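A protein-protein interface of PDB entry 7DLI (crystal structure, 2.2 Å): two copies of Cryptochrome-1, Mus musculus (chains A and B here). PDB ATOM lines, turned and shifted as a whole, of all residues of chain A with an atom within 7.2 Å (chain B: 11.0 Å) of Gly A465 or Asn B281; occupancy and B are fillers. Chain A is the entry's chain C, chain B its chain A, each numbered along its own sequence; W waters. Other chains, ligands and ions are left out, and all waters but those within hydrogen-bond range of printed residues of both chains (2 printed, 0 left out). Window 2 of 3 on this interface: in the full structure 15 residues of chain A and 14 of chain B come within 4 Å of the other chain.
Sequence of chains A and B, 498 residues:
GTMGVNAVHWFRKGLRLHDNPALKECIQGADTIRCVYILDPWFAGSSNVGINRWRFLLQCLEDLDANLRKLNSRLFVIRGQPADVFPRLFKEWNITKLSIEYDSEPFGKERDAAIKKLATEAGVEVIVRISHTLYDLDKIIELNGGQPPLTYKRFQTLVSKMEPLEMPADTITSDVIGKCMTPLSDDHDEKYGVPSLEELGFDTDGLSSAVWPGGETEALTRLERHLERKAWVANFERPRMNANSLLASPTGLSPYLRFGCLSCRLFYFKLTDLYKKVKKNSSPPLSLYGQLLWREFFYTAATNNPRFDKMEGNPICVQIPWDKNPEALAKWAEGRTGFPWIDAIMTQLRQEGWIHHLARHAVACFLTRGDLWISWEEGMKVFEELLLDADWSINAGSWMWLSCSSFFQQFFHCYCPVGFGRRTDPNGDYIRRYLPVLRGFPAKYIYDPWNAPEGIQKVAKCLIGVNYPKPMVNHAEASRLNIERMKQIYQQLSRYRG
O of Asn B281 lies close to O of Val A466.
O of Asn A467 sits close to N of Ser B283.
The side-chain amide nitrogen of Asn B281 lies close to the backbone carbonyl oxygen of Gly A465 (3.1 Å).
The backbone nitrogen of Pro A469 lies close to the backbone carbonyl oxygen of Asn B281 (3.2 Å).
The backbone carbonyl oxygen of Lys A331 sits at hydrogen-bond distance from the backbone NH of Arg A336, 2.9 Å away.
The backbone NH (N) of Leu A463 sits at hydrogen-bond distance from the side-chain amide oxygen (OD1) of Asn A467 (2.6 Å).
Arg A336 touches Lys B279.
Arg A336 touches Ser B282 (CD to OG, 3.4 Å).
C of Asn A467 touches O of Asn B281 (3.7 Å).
Asn A467 touches Ser B282 (O to C, 3.9 Å).
C of Tyr A468 touches O of Asn B281 (3.3 Å).
Pro A469 touches Ser B282 (CD to OG, 3.6 Å).
Of chain B, only Asn B281 (2.9 Å) comes within 4 Å of Gly A465.
Asn B281 touches just these residues of chain A: Gly A465 (2.9 Å), Val A466 (3.2 Å), Asn A467 (3.7 Å), Tyr A468 (3.3 Å) and Pro A469 (3.2 Å).
No residue of chain B comes within 4 Å of Ile A464.
Lys A470 touches none of the printed residues of chain B.
Of the printed residues of chain A, Ser B282 touches Arg A336, Asn A467 and Pro A469.
Of the printed residues of chain A, Ser B283 touches Asn A467 (3.1 Å).
Of the printed residues of chain B, Arg A336 touches Lys B279 (3.6 Å) and Ser B282 (3.4 Å).
Printed residues of chain A within 4 Å of Lys B279: Arg A336 (3.6 Å).
Of the printed residues of chain B, Asn A467 touches Asn B281 (3.7 Å), Ser B282 (3.9 Å) and Ser B283 (3.1 Å).
Leu B274 touches none of the printed residues of chain A.
Lys B280 touches none of the printed residues of chain A.
The nearest residue of chain B that does not touch Gly A465 is Lys B280 (6.1 Å).
The nearest residue of chain A that does not touch Asn B281 is Lys A470 (5.7 Å).
Of the 15 printed residues of chain B, 4 touch a printed residue of chain A.
Printed residues of chain B that touch a printed residue of chain A: Lys B279, Asn B281, Ser B282 and Ser B283.
Of the 12 printed residues of chain A, 6 touch a printed residue of chain B.
Printed residues of chain A that touch a printed residue of chain B: Arg A336, Gly A465, Val A466, Asn A467, Tyr A468 and Pro A469.
Among the printed residues, no Asp or Glu carboxylate lies within 4 Å of a Lys or Arg side-chain nitrogen of the other chain.
No position is printed for both chains.
Of the 10 pairs that touch across the chains among the printed residues, none has its exchanged pair printed and touching as well.
Water W2 lies within hydrogen-bond range of the side-chain hydroxyl (OG) of Ser B282 (2.6 Å), the backbone carbonyl oxygen (O) of Lys B280 (2.8 Å) and the guanidinium group (NH1) of Arg A336 (2.9 Å).
Water W1 lies within hydrogen-bond range of the side-chain amide nitrogen (ND2) of Asn B281 (3.0 Å) and the backbone NH (N) of Lys A470 (3.4 Å).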
ATOM      1  N   LYS A 331     -17.069 -10.535 -15.551  1.00  0.00           N
ATOM      2  CA  LYS A 331     -18.129  -9.618 -15.111  1.00  0.00           C
ATOM      3  C   LYS A 331     -18.390  -8.520 -16.145  1.00  0.00           C
ATOM      4  O   LYS A 331     -19.546  -8.160 -16.396  1.00  0.00           O
ATOM      5  CB  LYS A 331     -17.806  -9.021 -13.735  1.00  0.00           C
ATOM      6  CG  LYS A 331     -18.015 -10.015 -12.585  1.00  0.00           C
ATOM      7  CD  LYS A 331     -17.093  -9.735 -11.419  1.00  0.00           C
ATOM      8  CE  LYS A 331     -17.611  -8.639 -10.552  1.00  0.00           C
ATOM      9  NZ  LYS A 331     -18.637  -9.166  -9.594  1.00  0.00           N
ATOM     10  N   ARG A 336     -22.225  -7.883 -15.458  1.00  0.00           N
ATOM     11  CA  ARG A 336     -22.319  -8.076 -14.017  1.00  0.00           C
ATOM     12  C   ARG A 336     -21.340  -7.177 -13.273  1.00  0.00           C
ATOM     13  O   ARG A 336     -20.818  -7.559 -12.217  1.00  0.00           O
ATOM     14  CB  ARG A 336     -22.089  -9.551 -13.649  1.00  0.00           C
ATOM     15  CG  ARG A 336     -23.084 -10.525 -14.283  1.00  0.00           C
ATOM     16  CD  ARG A 336     -22.835 -12.005 -13.856  1.00  0.00           C
ATOM     17  NE  ARG A 336     -21.564 -12.579 -14.324  1.00  0.00           N
ATOM     18  CZ  ARG A 336     -20.515 -12.825 -13.537  1.00  0.00           C
ATOM     19  NH1 ARG A 336     -20.572 -12.541 -12.233  1.00  0.00           N
ATOM     20  NH2 ARG A 336     -19.399 -13.345 -14.049  1.00  0.00           N
ATOM     21  N   GLN A 457     -34.260  -0.071  -1.303  1.00  0.00           N
ATOM     22  CA  GLN A 457     -33.955  -1.344  -1.938  1.00  0.00           C
ATOM     23  C   GLN A 457     -35.091  -2.335  -1.728  1.00  0.00           C
ATOM     24  O   GLN A 457     -35.442  -3.086  -2.640  1.00  0.00           O
ATOM     25  CB  GLN A 457     -32.648  -1.895  -1.385  1.00  0.00           C
ATOM     26  CG  GLN A 457     -31.468  -1.025  -1.688  1.00  0.00           C
ATOM     27  CD  GLN A 457     -30.160  -1.653  -1.303  1.00  0.00           C
ATOM     28  OE1 GLN A 457     -30.030  -2.879  -1.267  1.00  0.00           O
ATOM     29  NE2 GLN A 457     -29.167  -0.813  -1.012  1.00  0.00           N
ATOM     30  N   CYS A 462     -35.109  -5.194  -4.819  1.00  0.00           N
ATOM     31  CA  CYS A 462     -33.795  -5.587  -5.306  1.00  0.00           C
ATOM     32  C   CYS A 462     -32.767  -5.203  -4.251  1.00  0.00           C
ATOM     33  O   CYS A 462     -32.516  -4.013  -4.039  1.00  0.00           O
ATOM     34  CB  CYS A 462     -33.502  -4.911  -6.648  1.00  0.00           C
ATOM     35  SG  CYS A 462     -31.882  -5.258  -7.308  1.00  0.00           S
ATOM     36  N   LEU A 463     -32.162  -6.193  -3.590  1.00  0.00           N
ATOM     37  CA  LEU A 463     -31.134  -5.925  -2.582  1.00  0.00           C
ATOM     38  C   LEU A 463     -29.753  -5.936  -3.241  1.00  0.00           C
ATOM     39  O   LEU A 463     -29.364  -6.928  -3.862  1.00  0.00           O
ATOM     40  CB  LEU A 463     -31.176  -6.963  -1.461  1.00  0.00           C
ATOM     41  CG  LEU A 463     -32.419  -7.007  -0.574  1.00  0.00           C
ATOM     42  CD1 LEU A 463     -32.337  -8.148   0.451  1.00  0.00           C
ATOM     43  CD2 LEU A 463     -32.583  -5.663   0.126  1.00  0.00           C
ATOM     44  N   ILE A 464     -29.015  -4.838  -3.116  1.00  0.00           N
ATOM     45  CA  ILE A 464     -27.682  -4.780  -3.716  1.00  0.00           C
ATOM     46  C   ILE A 464     -26.736  -5.677  -2.928  1.00  0.00           C
ATOM     47  O   ILE A 464     -26.626  -5.572  -1.698  1.00  0.00           O
ATOM     48  CB  ILE A 464     -27.159  -3.336  -3.783  1.00  0.00           C
ATOM     49  CG1 ILE A 464     -28.167  -2.448  -4.515  1.00  0.00           C
ATOM     50  CG2 ILE A 464     -25.851  -3.294  -4.535  1.00  0.00           C
ATOM     51  CD1 ILE A 464     -28.505  -2.968  -5.912  1.00  0.00           C
ATOM     52  N   GLY A 465     -26.024  -6.545  -3.636  1.00  0.00           N
ATOM     53  CA  GLY A 465     -25.240  -7.578  -3.010  1.00  0.00           C
ATOM     54  C   GLY A 465     -25.932  -8.917  -2.977  1.00  0.00           C
ATOM     55  O   GLY A 465     -25.308  -9.904  -2.574  1.00  0.00           O
ATOM     56  N   VAL A 466     -27.203  -8.977  -3.379  1.00  0.00           N
ATOM     57  CA  VAL A 466     -27.978 -10.215  -3.374  1.00  0.00           C
ATOM     58  C   VAL A 466     -28.582 -10.422  -4.757  1.00  0.00           C
ATOM     59  O   VAL A 466     -28.240 -11.381  -5.458  1.00  0.00           O
ATOM     60  CB  VAL A 466     -29.061 -10.194  -2.273  1.00  0.00           C
ATOM     61  CG1 VAL A 466     -29.966 -11.398  -2.371  1.00  0.00           C
ATOM     62  CG2 VAL A 466     -28.419 -10.146  -0.899  1.00  0.00           C
ATOM     63  N   ASN A 467     -29.552  -9.577  -5.120  1.00  0.00           N
ATOM     64  CA  ASN A 467     -30.225  -9.685  -6.416  1.00  0.00           C
ATOM     65  C   ASN A 467     -29.475  -9.010  -7.557  1.00  0.00           C
ATOM     66  O   ASN A 467     -29.710  -9.352  -8.717  1.00  0.00           O
ATOM     67  CB  ASN A 467     -31.623  -9.117  -6.309  1.00  0.00           C
ATOM     68  CG  ASN A 467     -32.293  -9.536  -5.030  1.00  0.00           C
ATOM     69  OD1 ASN A 467     -32.548  -8.715  -4.166  1.00  0.00           O
ATOM     70  ND2 ASN A 467     -32.563 -10.817  -4.897  1.00  0.00           N
ATOM     71  N   TYR A 468     -28.702  -7.965  -7.265  1.00  0.00           N
ATOM     72  CA  TYR A 468     -27.886  -7.246  -8.226  1.00  0.00           C
ATOM     73  C   TYR A 468     -26.554  -6.965  -7.541  1.00  0.00           C
ATOM     74  O   TYR A 468     -26.536  -6.556  -6.368  1.00  0.00           O
ATOM     75  CB  TYR A 468     -28.548  -5.931  -8.669  1.00  0.00           C
ATOM     76  CG  TYR A 468     -27.766  -5.174  -9.701  1.00  0.00           C
ATOM     77  CD1 TYR A 468     -27.765  -5.587 -11.022  1.00  0.00           C
ATOM     78  CD2 TYR A 468     -27.019  -4.054  -9.353  1.00  0.00           C
ATOM     79  CE1 TYR A 468     -27.051  -4.926 -11.969  1.00  0.00           C
ATOM     80  CE2 TYR A 468     -26.300  -3.360 -10.306  1.00  0.00           C
ATOM     81  CZ  TYR A 468     -26.321  -3.800 -11.615  1.00  0.00           C
ATOM     82  OH  TYR A 468     -25.595  -3.140 -12.576  1.00  0.00           O
ATOM     83  N   PRO A 469     -25.434  -7.158  -8.239  1.00  0.00           N
ATOM     84  CA  PRO A 469     -24.128  -7.058  -7.578  1.00  0.00           C
ATOM     85  C   PRO A 469     -23.735  -5.631  -7.222  1.00  0.00           C
ATOM     86  O   PRO A 469     -24.178  -4.652  -7.832  1.00  0.00           O
ATOM     87  CB  PRO A 469     -23.166  -7.659  -8.612  1.00  0.00           C
ATOM     88  CG  PRO A 469     -23.838  -7.417  -9.902  1.00  0.00           C
ATOM     89  CD  PRO A 469     -25.305  -7.628  -9.623  1.00  0.00           C
ATOM     90  N   LYS A 470     -22.882  -5.533  -6.204  1.00  0.00           N
ATOM     91  CA  LYS A 470     -22.237  -4.284  -5.852  1.00  0.00           C
ATOM     92  C   LYS A 470     -21.241  -3.886  -6.947  1.00  0.00           C
ATOM     93  O   LYS A 470     -20.731  -4.746  -7.673  1.00  0.00           O
ATOM     94  CB  LYS A 470     -21.506  -4.431  -4.523  1.00  0.00           C
ATOM     95  CG  LYS A 470     -22.404  -4.274  -3.322  1.00  0.00           C
ATOM     96  CD  LYS A 470     -21.712  -4.713  -2.058  1.00  0.00           C
ATOM     97  CE  LYS A 470     -22.649  -4.526  -0.862  1.00  0.00           C
ATOM     98  NZ  LYS A 470     -22.011  -3.717   0.218  1.00  0.00           N
ATOM     99  N   PHE B 236     -24.486 -21.608 -18.219  1.00  0.00           N
ATOM    100  CA  PHE B 236     -25.901 -21.271 -18.126  1.00  0.00           C
ATOM    101  C   PHE B 236     -26.482 -20.847 -19.465  1.00  0.00           C
ATOM    102  O   PHE B 236     -27.575 -20.272 -19.515  1.00  0.00           O
ATOM    103  CB  PHE B 236     -26.158 -20.195 -17.063  1.00  0.00           C
ATOM    104  CG  PHE B 236     -25.725 -20.592 -15.676  1.00  0.00           C
ATOM    105  CD1 PHE B 236     -26.551 -21.371 -14.864  1.00  0.00           C
ATOM    106  CD2 PHE B 236     -24.495 -20.180 -15.171  1.00  0.00           C
ATOM    107  CE1 PHE B 236     -26.169 -21.735 -13.581  1.00  0.00           C
ATOM    108  CE2 PHE B 236     -24.100 -20.535 -13.881  1.00  0.00           C
ATOM    109  CZ  PHE B 236     -24.940 -21.323 -13.088  1.00  0.00           C
ATOM    110  N   THR B 272     -31.645 -21.327  -9.601  1.00  0.00           N
ATOM    111  CA  THR B 272     -31.346 -19.970  -9.156  1.00  0.00           C
ATOM    112  C   THR B 272     -30.158 -19.950  -8.204  1.00  0.00           C
ATOM    113  O   THR B 272     -29.237 -19.136  -8.350  1.00  0.00           O
ATOM    114  CB  THR B 272     -32.580 -19.372  -8.460  1.00  0.00           C
ATOM    115  OG1 THR B 272     -33.740 -19.530  -9.284  1.00  0.00           O
ATOM    116  CG2 THR B 272     -32.378 -17.894  -8.131  1.00  0.00           C
ATOM    117  N   ASP B 273     -30.151 -20.867  -7.235  1.00  0.00           N
ATOM    118  CA  ASP B 273     -29.088 -20.887  -6.237  1.00  0.00           C
ATOM    119  C   ASP B 273     -27.742 -21.177  -6.867  1.00  0.00           C
ATOM    120  O   ASP B 273     -26.729 -20.585  -6.477  1.00  0.00           O
ATOM    121  CB  ASP B 273     -29.409 -21.899  -5.144  1.00  0.00           C
ATOM    122  CG  ASP B 273     -30.155 -21.269  -3.987  1.00  0.00           C
ATOM    123  OD1 ASP B 273     -29.835 -20.110  -3.640  1.00  0.00           O
ATOM    124  OD2 ASP B 273     -31.079 -21.914  -3.437  1.00  0.00           O
ATOM    125  N   LEU B 274     -27.709 -22.113  -7.818  1.00  0.00           N
ATOM    126  CA  LEU B 274     -26.475 -22.429  -8.523  1.00  0.00           C
ATOM    127  C   LEU B 274     -25.993 -21.247  -9.363  1.00  0.00           C
ATOM    128  O   LEU B 274     -24.790 -20.988  -9.432  1.00  0.00           O
ATOM    129  CB  LEU B 274     -26.692 -23.669  -9.382  1.00  0.00           C
ATOM    130  CG  LEU B 274     -25.465 -24.353  -9.968  1.00  0.00           C
ATOM    131  CD1 LEU B 274     -24.511 -24.764  -8.854  1.00  0.00           C
ATOM    132  CD2 LEU B 274     -25.943 -25.577 -10.729  1.00  0.00           C
ATOM    133  N   TYR B 275     -26.915 -20.539 -10.024  1.00  0.00           N
ATOM    134  CA  TYR B 275     -26.542 -19.329 -10.749  1.00  0.00           C
ATOM    135  C   TYR B 275     -25.950 -18.280  -9.807  1.00  0.00           C
ATOM    136  O   TYR B 275     -24.951 -17.626 -10.140  1.00  0.00           O
ATOM    137  CB  TYR B 275     -27.761 -18.770 -11.485  1.00  0.00           C
ATOM    138  CG  TYR B 275     -27.463 -17.625 -12.446  1.00  0.00           C
ATOM    139  CD1 TYR B 275     -27.376 -16.309 -11.998  1.00  0.00           C
ATOM    140  CD2 TYR B 275     -27.282 -17.869 -13.799  1.00  0.00           C
ATOM    141  CE1 TYR B 275     -27.101 -15.264 -12.883  1.00  0.00           C
ATOM    142  CE2 TYR B 275     -27.012 -16.847 -14.687  1.00  0.00           C
ATOM    143  CZ  TYR B 275     -26.928 -15.550 -14.229  1.00  0.00           C
ATOM    144  OH  TYR B 275     -26.656 -14.560 -15.135  1.00  0.00           O
ATOM    145  N   LYS B 276     -26.566 -18.101  -8.628  1.00  0.00           N
ATOM    146  CA  LYS B 276     -26.066 -17.150  -7.636  1.00  0.00           C
ATOM    147  C   LYS B 276     -24.689 -17.547  -7.109  1.00  0.00           C
ATOM    148  O   LYS B 276     -23.881 -16.676  -6.771  1.00  0.00           O
ATOM    149  CB  LYS B 276     -27.066 -16.998  -6.486  1.00  0.00           C
ATOM    150  N   LYS B 277     -24.406 -18.848  -7.003  1.00  0.00           N
ATOM    151  CA  LYS B 277     -23.070 -19.259  -6.577  1.00  0.00           C
ATOM    152  C   LYS B 277     -22.034 -18.943  -7.652  1.00  0.00           C
ATOM    153  O   LYS B 277     -20.981 -18.360  -7.363  1.00  0.00           O
ATOM    154  CB  LYS B 277     -23.057 -20.746  -6.220  1.00  0.00           C
ATOM    155  N   VAL B 278     -22.333 -19.284  -8.904  1.00  0.00           N
ATOM    156  CA  VAL B 278     -21.351 -19.124  -9.971  1.00  0.00           C
ATOM    157  C   VAL B 278     -21.228 -17.654 -10.375  1.00  0.00           C
ATOM    158  O   VAL B 278     -20.129 -17.161 -10.642  1.00  0.00           O
ATOM    159  CB  VAL B 278     -21.723 -20.031 -11.159  1.00  0.00           C
ATOM    160  N   LYS B 279     -22.353 -16.964 -10.517  1.00  0.00           N
ATOM    161  CA  LYS B 279     -22.406 -15.538 -10.825  1.00  0.00           C
ATOM    162  C   LYS B 279     -22.692 -14.856  -9.491  1.00  0.00           C
ATOM    163  O   LYS B 279     -23.842 -14.795  -9.053  1.00  0.00           O
ATOM    164  CB  LYS B 279     -23.478 -15.258 -11.873  1.00  0.00           C
ATOM    165  CG  LYS B 279     -23.420 -16.218 -13.064  1.00  0.00           C
ATOM    166  CD  LYS B 279     -22.042 -16.136 -13.747  1.00  0.00           C
ATOM    167  CE  LYS B 279     -21.874 -17.126 -14.897  1.00  0.00           C
ATOM    168  NZ  LYS B 279     -20.534 -16.964 -15.588  1.00  0.00           N
ATOM    169  N   LYS B 280     -21.649 -14.366  -8.829  1.00  0.00           N
ATOM    170  CA  LYS B 280     -21.794 -13.853  -7.469  1.00  0.00           C
ATOM    171  C   LYS B 280     -22.800 -12.719  -7.325  1.00  0.00           C
ATOM    172  O   LYS B 280     -22.565 -11.598  -7.790  1.00  0.00           O
ATOM    173  CB  LYS B 280     -20.443 -13.390  -6.925  1.00  0.00           C
ATOM    174  N   ASN B 281     -23.928 -13.019  -6.678  1.00  0.00           N
ATOM    175  CA  ASN B 281     -24.929 -12.019  -6.317  1.00  0.00           C
ATOM    176  C   ASN B 281     -25.587 -11.390  -7.534  1.00  0.00           C
ATOM    177  O   ASN B 281     -26.023 -10.242  -7.487  1.00  0.00           O
ATOM    178  CB  ASN B 281     -24.320 -10.953  -5.406  1.00  0.00           C
ATOM    179  CG  ASN B 281     -23.600 -11.572  -4.219  1.00  0.00           C
ATOM    180  OD1 ASN B 281     -23.994 -12.647  -3.754  1.00  0.00           O
ATOM    181  ND2 ASN B 281     -22.566 -10.904  -3.718  1.00  0.00           N
ATOM    182  N   SER B 282     -25.639 -12.118  -8.642  1.00  0.00           N
ATOM    183  CA  SER B 282     -26.373 -11.658  -9.807  1.00  0.00           C
ATOM    184  C   SER B 282     -27.659 -12.461  -9.934  1.00  0.00           C
ATOM    185  O   SER B 282     -27.672 -13.681  -9.743  1.00  0.00           O
ATOM    186  CB  SER B 282     -25.556 -11.773 -11.094  1.00  0.00           C
ATOM    187  OG  SER B 282     -24.550 -10.766 -11.157  1.00  0.00           O
ATOM    188  N   SER B 283     -28.719 -11.775 -10.296  1.00  0.00           N
ATOM    189  CA  SER B 283     -29.942 -12.523 -10.450  1.00  0.00           C
ATOM    190  C   SER B 283     -30.067 -12.885 -11.920  1.00  0.00           C
ATOM    191  O   SER B 283     -29.673 -12.099 -12.788  1.00  0.00           O
ATOM    192  CB  SER B 283     -31.159 -11.709 -10.002  1.00  0.00           C
ATOM    193  N   PRO B 284     -30.529 -14.110 -12.165  1.00  0.00           N
ATOM    194  CA  PRO B 284     -30.495 -14.652 -13.523  1.00  0.00           C
ATOM    195  C   PRO B 284     -31.552 -14.032 -14.416  1.00  0.00           C
ATOM    196  O   PRO B 284     -32.625 -13.614 -13.945  1.00  0.00           O
ATOM    197  CB  PRO B 284     -30.757 -16.152 -13.307  1.00  0.00           C
ATOM    198  CG  PRO B 284     -31.422 -16.228 -11.981  1.00  0.00           C
ATOM    199  CD  PRO B 284     -30.851 -15.130 -11.156  1.00  0.00           C
ATOM    200  N   PRO B 285     -31.298 -13.970 -15.723  1.00  0.00           N
ATOM    201  CA  PRO B 285     -32.337 -13.564 -16.675  1.00  0.00           C
ATOM    202  C   PRO B 285     -33.412 -14.629 -16.781  1.00  0.00           C
ATOM    203  O   PRO B 285     -33.152 -15.817 -16.579  1.00  0.00           O
ATOM    204  CB  PRO B 285     -31.568 -13.434 -17.997  1.00  0.00           C
ATOM    205  CG  PRO B 285     -30.465 -14.463 -17.864  1.00  0.00           C
ATOM    206  CD  PRO B 285     -30.067 -14.418 -16.406  1.00  0.00           C
HETATM  207  O   HOH W   1     -21.620  -8.312  -4.783  1.00  0.00           O
HETATM  208  O   HOH W   2     -22.087 -10.809 -10.443  1.00  0.00           O
